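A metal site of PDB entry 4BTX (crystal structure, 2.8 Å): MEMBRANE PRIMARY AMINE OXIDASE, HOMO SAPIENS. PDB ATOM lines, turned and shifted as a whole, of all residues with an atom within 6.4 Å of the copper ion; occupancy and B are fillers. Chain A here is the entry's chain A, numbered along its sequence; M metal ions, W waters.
The backbone NH (N) of Phe 656 is in hydrogen-bond range of the backbone carbonyl oxygen (O) of His 496, at 2.9 Å. A ring nitrogen (NE2) of His 658 sits at hydrogen-bond distance from the side-chain carboxylate of Asp 664 (2.6 Å).
Water W1 lies within hydrogen-bond range of OG1 of Thr 668, O2 of TPQ 445 and O of Tyr 468.
Along chain A the residues within 4 Å of the copper ion span positions 494 to 658. The nearest printed residue that does not touch the copper ion is TPQ 445 (4.7 Å).
The copper ion is bound by NE2 of His 494, ND1 of His 658 and NE2 of His 496. The copper ion has three donor atoms within binding distance.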
ATOM      1  N   TYR A 346      31.153 -28.691  21.844  1.00  0.00           N
ATOM      2  CA  TYR A 346      30.008 -28.192  22.560  1.00  0.00           C
ATOM      3  C   TYR A 346      30.079 -28.581  24.022  1.00  0.00           C
ATOM      4  O   TYR A 346      30.710 -29.574  24.410  1.00  0.00           O
ATOM      5  CB  TYR A 346      28.718 -28.734  21.930  1.00  0.00           C
ATOM      6  CG  TYR A 346      28.291 -27.931  20.753  1.00  0.00           C
ATOM      7  CD1 TYR A 346      28.751 -28.233  19.475  1.00  0.00           C
ATOM      8  CD2 TYR A 346      27.446 -26.858  20.915  1.00  0.00           C
ATOM      9  CE1 TYR A 346      28.367 -27.462  18.383  1.00  0.00           C
ATOM     10  CE2 TYR A 346      27.064 -26.081  19.835  1.00  0.00           C
ATOM     11  CZ  TYR A 346      27.527 -26.377  18.570  1.00  0.00           C
ATOM     12  OH  TYR A 346      27.108 -25.572  17.532  1.00  0.00           O
ATOM     13  N   TPQ A 445      25.211 -24.129  10.711  1.00  0.00           N
ATOM     14  CA  TPQ A 445      26.377 -23.271  10.458  1.00  0.00           C
ATOM     15  CB  TPQ A 445      27.705 -23.975  10.665  1.00  0.00           C
ATOM     16  C   TPQ A 445      26.397 -22.801   9.052  1.00  0.00           C
ATOM     17  O   TPQ A 445      26.140 -23.549   8.132  1.00  0.00           O
ATOM     18  C1  TPQ A 445      27.820 -24.821  11.923  1.00  0.00           C
ATOM     19  C2  TPQ A 445      27.841 -24.181  13.269  1.00  0.00           C
ATOM     20  O2  TPQ A 445      27.760 -22.929  13.429  1.00  0.00           O
ATOM     21  C3  TPQ A 445      27.952 -24.992  14.370  1.00  0.00           C
ATOM     22  C4  TPQ A 445      28.070 -26.377  14.239  1.00  0.00           C
ATOM     23  O4  TPQ A 445      28.157 -27.097  15.390  1.00  0.00           O
ATOM     24  C5  TPQ A 445      28.063 -27.046  12.896  1.00  0.00           C
ATOM     25  O5  TPQ A 445      28.159 -28.321  12.751  1.00  0.00           O
ATOM     26  C6  TPQ A 445      27.944 -26.209  11.784  1.00  0.00           C
ATOM     27  N   ALA A 465      32.118 -17.537  10.686  1.00  0.00           N
ATOM     28  CA  ALA A 465      30.977 -18.439  10.977  1.00  0.00           C
ATOM     29  C   ALA A 465      29.736 -17.597  11.226  1.00  0.00           C
ATOM     30  O   ALA A 465      29.776 -16.648  12.020  1.00  0.00           O
ATOM     31  CB  ALA A 465      31.273 -19.333  12.158  1.00  0.00           C
ATOM     32  N   TYR A 468      22.631 -19.938  11.767  1.00  0.00           N
ATOM     33  CA  TYR A 468      21.957 -20.204  12.996  1.00  0.00           C
ATOM     34  C   TYR A 468      22.982 -20.821  13.972  1.00  0.00           C
ATOM     35  O   TYR A 468      24.166 -20.950  13.657  1.00  0.00           O
ATOM     36  CB  TYR A 468      20.729 -21.113  12.717  1.00  0.00           C
ATOM     37  CG  TYR A 468      19.487 -20.350  12.261  1.00  0.00           C
ATOM     38  CD1 TYR A 468      18.611 -19.795  13.183  1.00  0.00           C
ATOM     39  CD2 TYR A 468      19.178 -20.201  10.922  1.00  0.00           C
ATOM     40  CE1 TYR A 468      17.475 -19.095  12.774  1.00  0.00           C
ATOM     41  CE2 TYR A 468      18.028 -19.504  10.517  1.00  0.00           C
ATOM     42  CZ  TYR A 468      17.184 -18.947  11.448  1.00  0.00           C
ATOM     43  OH  TYR A 468      16.047 -18.249  11.064  1.00  0.00           O
ATOM     44  N   ILE A 469      22.441 -21.200  15.132  1.00  0.00           N
ATOM     45  CA  ILE A 469      23.111 -21.532  16.372  1.00  0.00           C
ATOM     46  C   ILE A 469      22.488 -22.873  16.737  1.00  0.00           C
ATOM     47  O   ILE A 469      21.269 -22.971  16.673  1.00  0.00           O
ATOM     48  CB  ILE A 469      22.652 -20.494  17.436  1.00  0.00           C
ATOM     49  CG1 ILE A 469      22.717 -19.064  16.848  1.00  0.00           C
ATOM     50  CG2 ILE A 469      23.387 -20.627  18.739  1.00  0.00           C
ATOM     51  CD1 ILE A 469      21.509 -18.616  15.968  1.00  0.00           C
ATOM     52  N   HIS A 494      30.260 -23.391  22.747  1.00  0.00           N
ATOM     53  CA  HIS A 494      31.060 -24.232  21.859  1.00  0.00           C
ATOM     54  C   HIS A 494      32.286 -23.437  21.378  1.00  0.00           C
ATOM     55  O   HIS A 494      32.289 -22.178  21.385  1.00  0.00           O
ATOM     56  CB  HIS A 494      30.223 -24.686  20.659  1.00  0.00           C
ATOM     57  CG  HIS A 494      29.749 -23.550  19.822  1.00  0.00           C
ATOM     58  ND1 HIS A 494      28.684 -22.751  20.174  1.00  0.00           N
ATOM     59  CD2 HIS A 494      30.254 -23.004  18.688  1.00  0.00           C
ATOM     60  CE1 HIS A 494      28.528 -21.797  19.269  1.00  0.00           C
ATOM     61  NE2 HIS A 494      29.462 -21.932  18.359  1.00  0.00           N
ATOM     62  N   HIS A 496      34.804 -23.087  17.946  1.00  0.00           N
ATOM     63  CA  HIS A 496      35.088 -23.344  16.540  1.00  0.00           C
ATOM     64  C   HIS A 496      36.588 -23.378  16.270  1.00  0.00           C
ATOM     65  O   HIS A 496      37.305 -22.496  16.701  1.00  0.00           O
ATOM     66  CB  HIS A 496      34.596 -22.192  15.699  1.00  0.00           C
ATOM     67  CG  HIS A 496      33.128 -22.021  15.704  1.00  0.00           C
ATOM     68  ND1 HIS A 496      32.252 -23.027  15.352  1.00  0.00           N
ATOM     69  CD2 HIS A 496      32.351 -20.936  15.957  1.00  0.00           C
ATOM     70  CE1 HIS A 496      31.013 -22.580  15.417  1.00  0.00           C
ATOM     71  NE2 HIS A 496      31.052 -21.315  15.776  1.00  0.00           N
ATOM     72  N   PHE A 656      38.111 -19.967  17.749  1.00  0.00           N
ATOM     73  CA  PHE A 656      37.658 -19.125  18.845  1.00  0.00           C
ATOM     74  C   PHE A 656      36.487 -19.717  19.602  1.00  0.00           C
ATOM     75  O   PHE A 656      35.686 -20.423  19.029  1.00  0.00           O
ATOM     76  CB  PHE A 656      37.204 -17.781  18.319  1.00  0.00           C
ATOM     77  CG  PHE A 656      36.056 -17.847  17.392  1.00  0.00           C
ATOM     78  CD1 PHE A 656      36.250 -18.155  16.059  1.00  0.00           C
ATOM     79  CD2 PHE A 656      34.780 -17.581  17.837  1.00  0.00           C
ATOM     80  CE1 PHE A 656      35.171 -18.207  15.174  1.00  0.00           C
ATOM     81  CE2 PHE A 656      33.696 -17.616  16.969  1.00  0.00           C
ATOM     82  CZ  PHE A 656      33.893 -17.933  15.640  1.00  0.00           C
ATOM     83  N   HIS A 658      32.920 -19.527  21.349  1.00  0.00           N
ATOM     84  CA  HIS A 658      31.616 -18.887  21.134  1.00  0.00           C
ATOM     85  C   HIS A 658      30.654 -19.227  22.295  1.00  0.00           C
ATOM     86  O   HIS A 658      30.263 -20.399  22.499  1.00  0.00           O
ATOM     87  CB  HIS A 658      31.011 -19.353  19.823  1.00  0.00           C
ATOM     88  CG  HIS A 658      29.790 -18.602  19.408  1.00  0.00           C
ATOM     89  ND1 HIS A 658      29.209 -18.759  18.159  1.00  0.00           N
ATOM     90  CD2 HIS A 658      29.042 -17.679  20.045  1.00  0.00           C
ATOM     91  CE1 HIS A 658      28.163 -17.967  18.061  1.00  0.00           C
ATOM     92  NE2 HIS A 658      28.025 -17.313  19.188  1.00  0.00           N
ATOM     93  N   PRO A 660      27.125 -18.203  23.123  1.00  0.00           N
ATOM     94  CA  PRO A 660      26.099 -17.518  22.376  1.00  0.00           C
ATOM     95  C   PRO A 660      25.324 -16.514  23.209  1.00  0.00           C
ATOM     96  O   PRO A 660      25.337 -16.590  24.408  1.00  0.00           O
ATOM     97  CB  PRO A 660      25.195 -18.650  21.921  1.00  0.00           C
ATOM     98  CG  PRO A 660      26.035 -19.887  22.024  1.00  0.00           C
ATOM     99  CD  PRO A 660      26.940 -19.658  23.170  1.00  0.00           C
ATOM    100  N   ASP A 664      23.091 -13.202  18.558  1.00  0.00           N
ATOM    101  CA  ASP A 664      23.139 -14.357  17.659  1.00  0.00           C
ATOM    102  C   ASP A 664      21.719 -14.825  17.195  1.00  0.00           C
ATOM    103  O   ASP A 664      21.572 -15.895  16.564  1.00  0.00           O
ATOM    104  CB  ASP A 664      23.851 -15.535  18.335  1.00  0.00           C
ATOM    105  CG  ASP A 664      25.329 -15.256  18.645  1.00  0.00           C
ATOM    106  OD1 ASP A 664      25.947 -14.401  17.988  1.00  0.00           O
ATOM    107  OD2 ASP A 664      25.878 -15.945  19.550  1.00  0.00           O
ATOM    108  N   THR A 668      24.013 -15.640  14.151  1.00  0.00           N
ATOM    109  CA  THR A 668      25.396 -15.228  14.442  1.00  0.00           C
ATOM    110  C   THR A 668      25.883 -14.337  13.322  1.00  0.00           C
ATOM    111  O   THR A 668      25.646 -14.584  12.164  1.00  0.00           O
ATOM    112  CB  THR A 668      26.361 -16.406  14.494  1.00  0.00           C
ATOM    113  OG1 THR A 668      25.823 -17.476  15.311  1.00  0.00           O
ATOM    114  CG2 THR A 668      27.702 -15.950  15.066  1.00  0.00           C
ATOM    115  N   ASN A 673      33.951 -12.017  14.179  1.00  0.00           N
ATOM    116  CA  ASN A 673      34.114 -13.478  14.082  1.00  0.00           C
ATOM    117  C   ASN A 673      35.105 -13.949  13.013  1.00  0.00           C
ATOM    118  O   ASN A 673      35.251 -15.164  12.816  1.00  0.00           O
ATOM    119  CB  ASN A 673      32.753 -14.148  13.823  1.00  0.00           C
ATOM    120  CG  ASN A 673      31.912 -14.247  15.088  1.00  0.00           C
ATOM    121  OD1 ASN A 673      32.467 -13.761  16.203  1.00  0.00           O
ATOM    122  ND2 ASN A 673      30.792 -14.781  15.060  1.00  0.00           N
HETATM  123 CU    CU M   1      29.379 -20.440  17.025  1.00  0.00          CU
HETATM  124  O   HOH W   1      27.247 -20.086  14.737  1.00  0.00           O
